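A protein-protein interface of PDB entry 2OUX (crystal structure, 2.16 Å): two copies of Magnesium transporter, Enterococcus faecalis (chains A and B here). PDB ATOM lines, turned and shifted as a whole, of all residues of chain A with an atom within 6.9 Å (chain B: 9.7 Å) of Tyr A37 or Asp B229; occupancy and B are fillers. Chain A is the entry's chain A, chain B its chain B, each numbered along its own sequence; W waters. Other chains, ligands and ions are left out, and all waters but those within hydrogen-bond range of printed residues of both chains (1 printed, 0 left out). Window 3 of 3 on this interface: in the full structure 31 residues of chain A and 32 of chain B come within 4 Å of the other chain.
No position is printed for both chains.
Of the 7 pairs that touch across the chains among the printed residues, none has its exchanged pair printed and touching as well.
Water W1 lies within hydrogen-bond range of OD2 of Asp B231 (2.8 Å), O of Asp B229 (2.9 Å) and NE2 of His A35 (3.3 Å).
Among the printed residues, pairs that only touch across the chains: Met A8 with Tyr B230 (3.7 Å), His A35 with Phe B232 (3.8 Å), Tyr A37 with Tyr B230 (3.9 Å) and Val A69 with Asp B231 (3.6 Å).
OE2 of Glu A38 lies within hydrogen-bond range of OH of Tyr B230, 3.1 Å away.
The side-chain carboxylate (OD2) of Asp B229 is in hydrogen-bond range of the side-chain hydroxyl (OH) of Tyr A37 (3.4 Å).
A ring nitrogen (NE2) of His A35 sits close to the backbone carbonyl oxygen (O) of Tyr B230 (3.2 Å).
His A35 touches two residues of chain B.
No residue of chain B comes within 4 Å of Ile A36.
Tyr A37 touches just these residues of chain B: Asp B229 and Tyr B230.
No residue of chain B comes within 4 Å of Gly A40.
Of the printed residues of chain B, Val A69 touches Asp B231 (3.6 Å).
Printed residues of chain A within 4 Å of Tyr B230: Met A8, His A35, Tyr A37 and Glu A38.
Of the printed residues of chain A, Asp B231 touches Val A69.
The nearest residue of chain A that does not touch Asp B229 is His A35 (4.7 Å).
The nearest printed residue of chain A that does not touch Asp B231 is His A35 (4.9 Å).
Of the 17 printed residues of chain B, 4 touch a printed residue of chain A.
Hydrophobic or aromatic side chains of chain B within 4 Å of the printed part of chain A: Tyr B230 and Phe B232.
Hydrophobic or aromatic side chains of chain A that line the printed part of chain B: Met A8, His A35, Tyr A37 and Val A69.
Along chain A the printed residues that touch a printed residue of chain B span positions 8 to 69.
Among the printed residues, 7 pairs touch across the chains.
O of Ile B227 lies within hydrogen-bond range of N of Phe B232 (3.3 Å).
The side-chain amide nitrogen of Gln B225 is in hydrogen-bond range of the side-chain carboxylate of Asp B229, 3.4 Å away.
OE1 of Glu A38 sits at hydrogen-bond distance from N of His A35, at 3.4 Å.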
ATOM      1  N   MET A   8       3.102 -10.916 -14.112  1.00  0.00           N
ATOM      2  CA  MET A   8       1.922 -11.748 -13.949  1.00  0.00           C
ATOM      3  C   MET A   8       0.856 -11.061 -13.112  1.00  0.00           C
ATOM      4  O   MET A   8      -0.316 -11.023 -13.488  1.00  0.00           O
ATOM      5  CB  MET A   8       2.309 -13.064 -13.279  1.00  0.00           C
ATOM      6  CG  MET A   8       1.352 -14.185 -13.577  1.00  0.00           C
ATOM      7  SD  MET A   8       1.259 -14.361 -15.478  1.00  0.00           S
ATOM      8  CE  MET A   8       2.943 -15.260 -15.747  1.00  0.00           C
ATOM      9  N   PHE A  12      -3.093 -10.257 -14.244  1.00  0.00           N
ATOM     10  CA  PHE A  12      -4.159 -10.946 -13.530  1.00  0.00           C
ATOM     11  C   PHE A  12      -5.144  -9.957 -12.905  1.00  0.00           C
ATOM     12  O   PHE A  12      -6.353 -10.178 -12.935  1.00  0.00           O
ATOM     13  CB  PHE A  12      -3.571 -11.858 -12.447  1.00  0.00           C
ATOM     14  CG  PHE A  12      -3.030 -13.167 -12.971  1.00  0.00           C
ATOM     15  CD1 PHE A  12      -2.943 -13.413 -14.342  1.00  0.00           C
ATOM     16  CD2 PHE A  12      -2.612 -14.157 -12.093  1.00  0.00           C
ATOM     17  CE1 PHE A  12      -2.451 -14.625 -14.824  1.00  0.00           C
ATOM     18  CE2 PHE A  12      -2.117 -15.375 -12.568  1.00  0.00           C
ATOM     19  CZ  PHE A  12      -2.037 -15.606 -13.937  1.00  0.00           C
ATOM     20  N   LEU A  34      -3.228 -15.153 -22.870  1.00  0.00           N
ATOM     21  CA  LEU A  34      -2.314 -15.804 -21.938  1.00  0.00           C
ATOM     22  C   LEU A  34      -2.045 -17.237 -22.398  1.00  0.00           C
ATOM     23  O   LEU A  34      -2.906 -17.876 -22.997  1.00  0.00           O
ATOM     24  CB  LEU A  34      -2.931 -15.862 -20.534  1.00  0.00           C
ATOM     25  CG  LEU A  34      -3.267 -14.608 -19.725  1.00  0.00           C
ATOM     26  CD1 LEU A  34      -4.096 -15.007 -18.524  1.00  0.00           C
ATOM     27  CD2 LEU A  34      -1.992 -13.921 -19.274  1.00  0.00           C
ATOM     28  N   HIS A  35      -0.843 -17.725 -22.106  1.00  0.00           N
ATOM     29  CA  HIS A  35      -0.445 -19.097 -22.414  1.00  0.00           C
ATOM     30  C   HIS A  35      -1.318 -19.966 -21.495  1.00  0.00           C
ATOM     31  O   HIS A  35      -1.635 -19.549 -20.389  1.00  0.00           O
ATOM     32  CB  HIS A  35       1.037 -19.278 -22.069  1.00  0.00           C
ATOM     33  CG  HIS A  35       1.523 -20.689 -22.191  1.00  0.00           C
ATOM     34  ND1 HIS A  35       2.337 -21.110 -23.226  1.00  0.00           N
ATOM     35  CD2 HIS A  35       1.328 -21.766 -21.401  1.00  0.00           C
ATOM     36  CE1 HIS A  35       2.620 -22.389 -23.062  1.00  0.00           C
ATOM     37  NE2 HIS A  35       2.023 -22.814 -21.965  1.00  0.00           N
ATOM     38  N   ILE A  36      -1.701 -21.159 -21.937  1.00  0.00           N
ATOM     39  CA  ILE A  36      -2.556 -22.018 -21.122  1.00  0.00           C
ATOM     40  C   ILE A  36      -2.085 -22.263 -19.690  1.00  0.00           C
ATOM     41  O   ILE A  36      -2.909 -22.497 -18.814  1.00  0.00           O
ATOM     42  CB  ILE A  36      -2.813 -23.382 -21.793  1.00  0.00           C
ATOM     43  CG1 ILE A  36      -1.490 -24.026 -22.210  1.00  0.00           C
ATOM     44  CG2 ILE A  36      -3.765 -23.206 -22.972  1.00  0.00           C
ATOM     45  CD1 ILE A  36      -1.632 -25.474 -22.636  1.00  0.00           C
ATOM     46  N   TYR A  37      -0.777 -22.212 -19.441  1.00  0.00           N
ATOM     47  CA  TYR A  37      -0.275 -22.409 -18.080  1.00  0.00           C
ATOM     48  C   TYR A  37      -0.600 -21.192 -17.217  1.00  0.00           C
ATOM     49  O   TYR A  37      -0.887 -21.326 -16.030  1.00  0.00           O
ATOM     50  CB  TYR A  37       1.234 -22.620 -18.052  1.00  0.00           C
ATOM     51  CG  TYR A  37       1.820 -22.459 -16.660  1.00  0.00           C
ATOM     52  CD1 TYR A  37       1.663 -23.453 -15.686  1.00  0.00           C
ATOM     53  CD2 TYR A  37       2.491 -21.293 -16.302  1.00  0.00           C
ATOM     54  CE1 TYR A  37       2.174 -23.286 -14.389  1.00  0.00           C
ATOM     55  CE2 TYR A  37       3.002 -21.114 -15.015  1.00  0.00           C
ATOM     56  CZ  TYR A  37       2.836 -22.110 -14.066  1.00  0.00           C
ATOM     57  OH  TYR A  37       3.349 -21.923 -12.806  1.00  0.00           O
ATOM     58  N   GLU A  38      -0.517 -20.007 -17.808  1.00  0.00           N
ATOM     59  CA  GLU A  38      -0.833 -18.788 -17.068  1.00  0.00           C
ATOM     60  C   GLU A  38      -2.353 -18.774 -16.843  1.00  0.00           C
ATOM     61  O   GLU A  38      -2.842 -18.324 -15.799  1.00  0.00           O
ATOM     62  CB  GLU A  38      -0.371 -17.551 -17.851  1.00  0.00           C
ATOM     63  CG  GLU A  38       1.102 -17.588 -18.211  1.00  0.00           C
ATOM     64  CD  GLU A  38       1.579 -16.361 -18.973  1.00  0.00           C
ATOM     65  OE1 GLU A  38       0.857 -15.866 -19.872  1.00  0.00           O
ATOM     66  OE2 GLU A  38       2.703 -15.902 -18.686  1.00  0.00           O
ATOM     67  N   GLN A  39      -3.093 -19.283 -17.825  1.00  0.00           N
ATOM     68  CA  GLN A  39      -4.547 -19.367 -17.710  1.00  0.00           C
ATOM     69  C   GLN A  39      -4.871 -20.233 -16.495  1.00  0.00           C
ATOM     70  O   GLN A  39      -5.789 -19.933 -15.730  1.00  0.00           O
ATOM     71  CB  GLN A  39      -5.155 -19.999 -18.968  1.00  0.00           C
ATOM     72  CG  GLN A  39      -5.197 -19.060 -20.173  1.00  0.00           C
ATOM     73  CD  GLN A  39      -5.650 -19.751 -21.445  1.00  0.00           C
ATOM     74  OE1 GLN A  39      -6.479 -20.664 -21.415  1.00  0.00           O
ATOM     75  NE2 GLN A  39      -5.103 -19.315 -22.577  1.00  0.00           N
ATOM     76  N   GLY A  40      -4.106 -21.307 -16.322  1.00  0.00           N
ATOM     77  CA  GLY A  40      -4.332 -22.193 -15.195  1.00  0.00           C
ATOM     78  C   GLY A  40      -4.075 -21.530 -13.850  1.00  0.00           C
ATOM     79  O   GLY A  40      -4.828 -21.723 -12.894  1.00  0.00           O
ATOM     80  N   GLN A  41      -3.006 -20.748 -13.763  1.00  0.00           N
ATOM     81  CA  GLN A  41      -2.677 -20.065 -12.522  1.00  0.00           C
ATOM     82  C   GLN A  41      -3.747 -19.035 -12.179  1.00  0.00           C
ATOM     83  O   GLN A  41      -4.198 -18.954 -11.035  1.00  0.00           O
ATOM     84  CB  GLN A  41      -1.308 -19.394 -12.641  1.00  0.00           C
ATOM     85  CG  GLN A  41      -0.180 -20.392 -12.837  1.00  0.00           C
ATOM     86  CD  GLN A  41      -0.139 -21.430 -11.729  1.00  0.00           C
ATOM     87  OE1 GLN A  41       0.246 -21.129 -10.600  1.00  0.00           O
ATOM     88  NE2 GLN A  41      -0.550 -22.656 -12.045  1.00  0.00           N
ATOM     89  N   PHE A  42      -4.145 -18.245 -13.171  1.00  0.00           N
ATOM     90  CA  PHE A  42      -5.181 -17.243 -12.967  1.00  0.00           C
ATOM     91  C   PHE A  42      -6.415 -17.946 -12.417  1.00  0.00           C
ATOM     92  O   PHE A  42      -6.921 -17.584 -11.360  1.00  0.00           O
ATOM     93  CB  PHE A  42      -5.538 -16.553 -14.287  1.00  0.00           C
ATOM     94  CG  PHE A  42      -6.687 -15.591 -14.173  1.00  0.00           C
ATOM     95  CD1 PHE A  42      -6.525 -14.363 -13.533  1.00  0.00           C
ATOM     96  CD2 PHE A  42      -7.936 -15.924 -14.678  1.00  0.00           C
ATOM     97  CE1 PHE A  42      -7.595 -13.481 -13.395  1.00  0.00           C
ATOM     98  CE2 PHE A  42      -9.008 -15.053 -14.545  1.00  0.00           C
ATOM     99  CZ  PHE A  42      -8.838 -13.824 -13.901  1.00  0.00           C
ATOM    100  N   GLN A  44      -6.796 -20.864 -10.981  1.00  0.00           N
ATOM    101  CA  GLN A  44      -6.626 -21.495  -9.678  1.00  0.00           C
ATOM    102  C   GLN A  44      -6.519 -20.481  -8.541  1.00  0.00           C
ATOM    103  O   GLN A  44      -6.341 -20.856  -7.386  1.00  0.00           O
ATOM    104  CB  GLN A  44      -5.392 -22.406  -9.695  1.00  0.00           C
ATOM    105  CG  GLN A  44      -5.586 -23.664 -10.529  1.00  0.00           C
ATOM    106  CD  GLN A  44      -4.321 -24.496 -10.656  1.00  0.00           C
ATOM    107  OE1 GLN A  44      -3.808 -25.035  -9.672  1.00  0.00           O
ATOM    108  NE2 GLN A  44      -3.808 -24.601 -11.876  1.00  0.00           N
ATOM    109  N   ASP A  65      -8.483 -26.607 -23.107  1.00  0.00           N
ATOM    110  CA  ASP A  65      -7.103 -26.263 -23.434  1.00  0.00           C
ATOM    111  C   ASP A  65      -6.345 -25.937 -22.154  1.00  0.00           C
ATOM    112  O   ASP A  65      -5.149 -26.213 -22.028  1.00  0.00           O
ATOM    113  CB  ASP A  65      -7.045 -25.036 -24.351  1.00  0.00           C
ATOM    114  CG  ASP A  65      -7.587 -25.310 -25.725  1.00  0.00           C
ATOM    115  OD1 ASP A  65      -7.304 -26.395 -26.268  1.00  0.00           O
ATOM    116  OD2 ASP A  65      -8.285 -24.428 -26.270  1.00  0.00           O
ATOM    117  N   MET A  66      -7.051 -25.328 -21.213  1.00  0.00           N
ATOM    118  CA  MET A  66      -6.431 -24.955 -19.961  1.00  0.00           C
ATOM    119  C   MET A  66      -6.300 -26.155 -19.030  1.00  0.00           C
ATOM    120  O   MET A  66      -5.231 -26.375 -18.455  1.00  0.00           O
ATOM    121  CB  MET A  66      -7.234 -23.848 -19.272  1.00  0.00           C
ATOM    122  CG  MET A  66      -6.695 -23.498 -17.892  1.00  0.00           C
ATOM    123  SD  MET A  66      -7.886 -22.391 -16.860  1.00  0.00           S
ATOM    124  CE  MET A  66      -9.309 -23.665 -16.608  1.00  0.00           C
ATOM    125  N   VAL A  69      -3.404 -28.726 -18.837  1.00  0.00           N
ATOM    126  CA  VAL A  69      -2.179 -28.531 -18.080  1.00  0.00           C
ATOM    127  C   VAL A  69      -2.295 -28.361 -16.575  1.00  0.00           C
ATOM    128  O   VAL A  69      -1.281 -28.320 -15.880  1.00  0.00           O
ATOM    129  CB  VAL A  69      -1.365 -27.364 -18.650  1.00  0.00           C
ATOM    130  CG1 VAL A  69      -1.003 -27.668 -20.097  1.00  0.00           C
ATOM    131  CG2 VAL A  69      -2.160 -26.063 -18.548  1.00  0.00           C
ATOM    132  N   ILE A  70      -3.517 -28.251 -16.067  1.00  0.00           N
ATOM    133  CA  ILE A  70      -3.710 -28.131 -14.628  1.00  0.00           C
ATOM    134  C   ILE A  70      -3.360 -29.517 -14.060  1.00  0.00           C
ATOM    135  O   ILE A  70      -3.780 -30.544 -14.602  1.00  0.00           O
ATOM    136  CB  ILE A  70      -5.200 -27.789 -14.269  1.00  0.00           C
ATOM    137  CG1 ILE A  70      -5.597 -26.434 -14.865  1.00  0.00           C
ATOM    138  CG2 ILE A  70      -5.381 -27.799 -12.759  1.00  0.00           C
ATOM    139  CD1 ILE A  70      -4.631 -25.312 -14.499  1.00  0.00           C
ATOM    140  N   GLU A  71      -2.586 -29.553 -12.983  1.00  0.00           N
ATOM    141  CA  GLU A  71      -2.205 -30.827 -12.382  1.00  0.00           C
ATOM    142  C   GLU A  71      -3.437 -31.596 -11.913  1.00  0.00           C
ATOM    143  O   GLU A  71      -4.118 -31.171 -10.989  1.00  0.00           O
ATOM    144  CB  GLU A  71      -1.239 -30.583 -11.222  1.00  0.00           C
ATOM    145  CG  GLU A  71       0.174 -30.274 -11.685  1.00  0.00           C
ATOM    146  CD  GLU A  71       1.082 -29.802 -10.559  1.00  0.00           C
ATOM    147  OE1 GLU A  71       1.142 -30.485  -9.514  1.00  0.00           O
ATOM    148  OE2 GLU A  71       1.742 -28.750 -10.718  1.00  0.00           O
ATOM    149  N   ILE B 212       7.735 -15.440 -23.619  1.00  0.00           N
ATOM    150  CA  ILE B 212       8.400 -15.857 -22.389  1.00  0.00           C
ATOM    151  C   ILE B 212       9.886 -16.046 -22.668  1.00  0.00           C
ATOM    152  O   ILE B 212      10.253 -16.672 -23.662  1.00  0.00           O
ATOM    153  CB  ILE B 212       7.827 -17.193 -21.861  1.00  0.00           C
ATOM    154  CG1 ILE B 212       6.333 -17.044 -21.549  1.00  0.00           C
ATOM    155  CG2 ILE B 212       8.588 -17.630 -20.618  1.00  0.00           C
ATOM    156  CD1 ILE B 212       5.445 -17.058 -22.785  1.00  0.00           C
ATOM    157  N   GLU B 221      18.204 -24.330 -12.979  1.00  0.00           N
ATOM    158  CA  GLU B 221      17.055 -24.887 -12.265  1.00  0.00           C
ATOM    159  C   GLU B 221      15.780 -24.082 -12.542  1.00  0.00           C
ATOM    160  O   GLU B 221      14.684 -24.639 -12.703  1.00  0.00           O
ATOM    161  CB  GLU B 221      17.353 -24.882 -10.762  1.00  0.00           C
ATOM    162  CG  GLU B 221      16.374 -25.663  -9.899  1.00  0.00           C
ATOM    163  CD  GLU B 221      16.975 -26.953  -9.363  1.00  0.00           C
ATOM    164  OE1 GLU B 221      16.700 -28.025  -9.943  1.00  0.00           O
ATOM    165  OE2 GLU B 221      17.730 -26.884  -8.366  1.00  0.00           O
ATOM    166  N   ASP B 222      15.926 -22.764 -12.573  1.00  0.00           N
ATOM    167  CA  ASP B 222      14.797 -21.889 -12.837  1.00  0.00           C
ATOM    168  C   ASP B 222      14.401 -22.009 -14.314  1.00  0.00           C
ATOM    169  O   ASP B 222      13.220 -21.943 -14.665  1.00  0.00           O
ATOM    170  CB  ASP B 222      15.162 -20.443 -12.474  1.00  0.00           C
ATOM    171  CG  ASP B 222      15.432 -20.268 -10.973  1.00  0.00           C
ATOM    172  OD1 ASP B 222      14.706 -20.885 -10.171  1.00  0.00           O
ATOM    173  OD2 ASP B 222      16.356 -19.508 -10.587  1.00  0.00           O
ATOM    174  N   VAL B 223      15.397 -22.194 -15.177  1.00  0.00           N
ATOM    175  CA  VAL B 223      15.130 -22.346 -16.600  1.00  0.00           C
ATOM    176  C   VAL B 223      14.379 -23.656 -16.784  1.00  0.00           C
ATOM    177  O   VAL B 223      13.431 -23.744 -17.559  1.00  0.00           O
ATOM    178  CB  VAL B 223      16.440 -22.395 -17.402  1.00  0.00           C
ATOM    179  CG1 VAL B 223      16.141 -22.623 -18.895  1.00  0.00           C
ATOM    180  CG2 VAL B 223      17.199 -21.092 -17.197  1.00  0.00           C
ATOM    181  N   ALA B 224      14.801 -24.670 -16.041  1.00  0.00           N
ATOM    182  CA  ALA B 224      14.169 -25.981 -16.114  1.00  0.00           C
ATOM    183  C   ALA B 224      12.711 -25.868 -15.687  1.00  0.00           C
ATOM    184  O   ALA B 224      11.826 -26.499 -16.273  1.00  0.00           O
ATOM    185  CB  ALA B 224      14.903 -26.949 -15.205  1.00  0.00           C
ATOM    186  N   GLN B 225      12.464 -25.067 -14.656  1.00  0.00           N
ATOM    187  CA  GLN B 225      11.100 -24.892 -14.168  1.00  0.00           C
ATOM    188  C   GLN B 225      10.199 -24.235 -15.222  1.00  0.00           C
ATOM    189  O   GLN B 225       9.061 -24.649 -15.416  1.00  0.00           O
ATOM    190  CB  GLN B 225      11.075 -24.044 -12.891  1.00  0.00           C
ATOM    191  CG  GLN B 225       9.712 -24.065 -12.192  1.00  0.00           C
ATOM    192  CD  GLN B 225       9.320 -25.467 -11.788  1.00  0.00           C
ATOM    193  OE1 GLN B 225      10.158 -26.238 -11.325  1.00  0.00           O
ATOM    194  NE2 GLN B 225       8.048 -25.807 -11.951  1.00  0.00           N
ATOM    195  N   THR B 226      10.719 -23.211 -15.893  1.00  0.00           N
ATOM    196  CA  THR B 226       9.963 -22.509 -16.919  1.00  0.00           C
ATOM    197  C   THR B 226       9.595 -23.446 -18.072  1.00  0.00           C
ATOM    198  O   THR B 226       8.478 -23.428 -18.552  1.00  0.00           O
ATOM    199  CB  THR B 226      10.772 -21.318 -17.478  1.00  0.00           C
ATOM    200  OG1 THR B 226      11.013 -20.374 -16.428  1.00  0.00           O
ATOM    201  CG2 THR B 226      10.012 -20.630 -18.621  1.00  0.00           C
ATOM    202  N   ILE B 227      10.537 -24.275 -18.503  1.00  0.00           N
ATOM    203  CA  ILE B 227      10.284 -25.190 -19.605  1.00  0.00           C
ATOM    204  C   ILE B 227       9.263 -26.252 -19.180  1.00  0.00           C
ATOM    205  O   ILE B 227       8.450 -26.713 -19.982  1.00  0.00           O
ATOM    206  CB  ILE B 227      11.603 -25.877 -20.078  1.00  0.00           C
ATOM    207  CG1 ILE B 227      12.390 -24.947 -21.014  1.00  0.00           C
ATOM    208  CG2 ILE B 227      11.267 -27.199 -20.758  1.00  0.00           C
ATOM    209  CD1 ILE B 227      11.701 -24.720 -22.354  1.00  0.00           C
ATOM    210  N   ARG B 228       9.327 -26.630 -17.909  1.00  0.00           N
ATOM    211  CA  ARG B 228       8.432 -27.614 -17.318  1.00  0.00           C
ATOM    212  C   ARG B 228       6.997 -27.060 -17.267  1.00  0.00           C
ATOM    213  O   ARG B 228       6.054 -27.720 -17.675  1.00  0.00           O
ATOM    214  CB  ARG B 228       8.964 -27.943 -15.913  1.00  0.00           C
ATOM    215  CG  ARG B 228       8.112 -28.821 -15.048  1.00  0.00           C
ATOM    216  CD  ARG B 228       8.796 -29.024 -13.693  1.00  0.00           C
ATOM    217  NE  ARG B 228       9.951 -29.923 -13.744  1.00  0.00           N
ATOM    218  CZ  ARG B 228      11.159 -29.623 -13.279  1.00  0.00           C
ATOM    219  NH1 ARG B 228      11.392 -28.442 -12.729  1.00  0.00           N
ATOM    220  NH2 ARG B 228      12.138 -30.514 -13.346  1.00  0.00           N
ATOM    221  N   ASP B 229       6.825 -25.834 -16.794  1.00  0.00           N
ATOM    222  CA  ASP B 229       5.485 -25.257 -16.707  1.00  0.00           C
ATOM    223  C   ASP B 229       4.818 -24.910 -18.039  1.00  0.00           C
ATOM    224  O   ASP B 229       3.655 -25.245 -18.264  1.00  0.00           O
ATOM    225  CB  ASP B 229       5.508 -24.010 -15.822  1.00  0.00           C
ATOM    226  CG  ASP B 229       5.684 -24.346 -14.357  1.00  0.00           C
ATOM    227  OD1 ASP B 229       5.267 -25.456 -13.956  1.00  0.00           O
ATOM    228  OD2 ASP B 229       6.219 -23.498 -13.610  1.00  0.00           O
ATOM    229  N   TYR B 230       5.552 -24.251 -18.926  1.00  0.00           N
ATOM    230  CA  TYR B 230       4.992 -23.848 -20.218  1.00  0.00           C
ATOM    231  C   TYR B 230       5.054 -24.907 -21.305  1.00  0.00           C
ATOM    232  O   TYR B 230       4.635 -24.651 -22.437  1.00  0.00           O
ATOM    233  CB  TYR B 230       5.709 -22.596 -20.718  1.00  0.00           C
ATOM    234  CG  TYR B 230       5.436 -21.371 -19.883  1.00  0.00           C
ATOM    235  CD1 TYR B 230       4.415 -20.476 -20.228  1.00  0.00           C
ATOM    236  CD2 TYR B 230       6.191 -21.104 -18.741  1.00  0.00           C
ATOM    237  CE1 TYR B 230       4.161 -19.342 -19.453  1.00  0.00           C
ATOM    238  CE2 TYR B 230       5.943 -19.976 -17.964  1.00  0.00           C
ATOM    239  CZ  TYR B 230       4.927 -19.099 -18.325  1.00  0.00           C
ATOM    240  OH  TYR B 230       4.691 -17.981 -17.555  1.00  0.00           O
ATOM    241  N   ASP B 231       5.571 -26.087 -20.964  1.00  0.00           N
ATOM    242  CA  ASP B 231       5.716 -27.184 -21.924  1.00  0.00           C
ATOM    243  C   ASP B 231       6.400 -26.730 -23.223  1.00  0.00           C
ATOM    244  O   ASP B 231       5.916 -27.017 -24.322  1.00  0.00           O
ATOM    245  CB  ASP B 231       4.350 -27.792 -22.245  1.00  0.00           C
ATOM    246  CG  ASP B 231       3.694 -28.374 -21.030  1.00  0.00           C
ATOM    247  OD1 ASP B 231       4.456 -28.845 -20.187  1.00  0.00           O
ATOM    248  OD2 ASP B 231       2.445 -28.371 -20.909  1.00  0.00           O
ATOM    249  N   PHE B 232       7.528 -26.028 -23.088  1.00  0.00           N
ATOM    250  CA  PHE B 232       8.253 -25.523 -24.249  1.00  0.00           C
ATOM    251  C   PHE B 232       9.281 -26.497 -24.793  1.00  0.00           C
ATOM    252  O   PHE B 232       9.891 -27.246 -24.036  1.00  0.00           O
ATOM    253  CB  PHE B 232       9.004 -24.225 -23.914  1.00  0.00           C
ATOM    254  CG  PHE B 232       8.117 -23.031 -23.681  1.00  0.00           C
ATOM    255  CD1 PHE B 232       6.948 -22.856 -24.413  1.00  0.00           C
ATOM    256  CD2 PHE B 232       8.512 -22.024 -22.792  1.00  0.00           C
ATOM    257  CE1 PHE B 232       6.189 -21.699 -24.268  1.00  0.00           C
ATOM    258  CE2 PHE B 232       7.764 -20.868 -22.645  1.00  0.00           C
ATOM    259  CZ  PHE B 232       6.600 -20.703 -23.387  1.00  0.00           C
ATOM    260  N   LEU B 233       9.485 -26.456 -26.108  1.00  0.00           N
ATOM    261  CA  LEU B 233      10.477 -27.290 -26.765  1.00  0.00           C
ATOM    262  C   LEU B 233      11.776 -26.536 -26.611  1.00  0.00           C
ATOM    263  O   LEU B 233      12.849 -27.122 -26.630  1.00  0.00           O
ATOM    264  CB  LEU B 233      10.182 -27.444 -28.255  1.00  0.00           C
ATOM    265  CG  LEU B 233       8.881 -28.114 -28.683  1.00  0.00           C
ATOM    266  CD1 LEU B 233       8.746 -28.060 -30.198  1.00  0.00           C
ATOM    267  CD2 LEU B 233       8.861 -29.546 -28.180  1.00  0.00           C
ATOM    268  N   VAL B 250      14.724 -28.251 -24.819  1.00  0.00           N
ATOM    269  CA  VAL B 250      14.203 -29.256 -23.903  1.00  0.00           C
ATOM    270  C   VAL B 250      15.072 -30.504 -23.725  1.00  0.00           C
ATOM    271  O   VAL B 250      15.188 -31.025 -22.614  1.00  0.00           O
ATOM    272  CB  VAL B 250      12.751 -29.660 -24.315  1.00  0.00           C
ATOM    273  CG1 VAL B 250      12.752 -30.466 -25.627  1.00  0.00           C
ATOM    274  CG2 VAL B 250      12.085 -30.408 -23.191  1.00  0.00           C
ATOM    275  N   ILE B 253      17.621 -29.577 -21.256  1.00  0.00           N
ATOM    276  CA  ILE B 253      17.073 -29.287 -19.945  1.00  0.00           C
ATOM    277  C   ILE B 253      16.837 -30.609 -19.214  1.00  0.00           C
ATOM    278  O   ILE B 253      16.927 -30.667 -17.989  1.00  0.00           O
ATOM    279  CB  ILE B 253      15.752 -28.458 -20.052  1.00  0.00           C
ATOM    280  CG1 ILE B 253      16.081 -26.965 -19.973  1.00  0.00           C
ATOM    281  CG2 ILE B 253      14.767 -28.869 -18.961  1.00  0.00           C
ATOM    282  CD1 ILE B 253      16.711 -26.549 -18.667  1.00  0.00           C
ATOM    283  N   ILE B 257      17.998 -31.595 -15.534  1.00  0.00           N
ATOM    284  CA  ILE B 257      17.091 -32.133 -14.540  1.00  0.00           C
ATOM    285  C   ILE B 257      17.654 -33.436 -13.965  1.00  0.00           C
ATOM    286  O   ILE B 257      17.605 -33.658 -12.759  1.00  0.00           O
ATOM    287  CB  ILE B 257      15.680 -32.359 -15.151  1.00  0.00           C
ATOM    288  CG1 ILE B 257      15.096 -31.028 -15.637  1.00  0.00           C
ATOM    289  CG2 ILE B 257      14.746 -32.949 -14.111  1.00  0.00           C
ATOM    290  CD1 ILE B 257      14.862 -30.046 -14.525  1.00  0.00           C
HETATM  291  O   HOH W   1       1.825 -25.695 -20.422  1.00  0.00           O
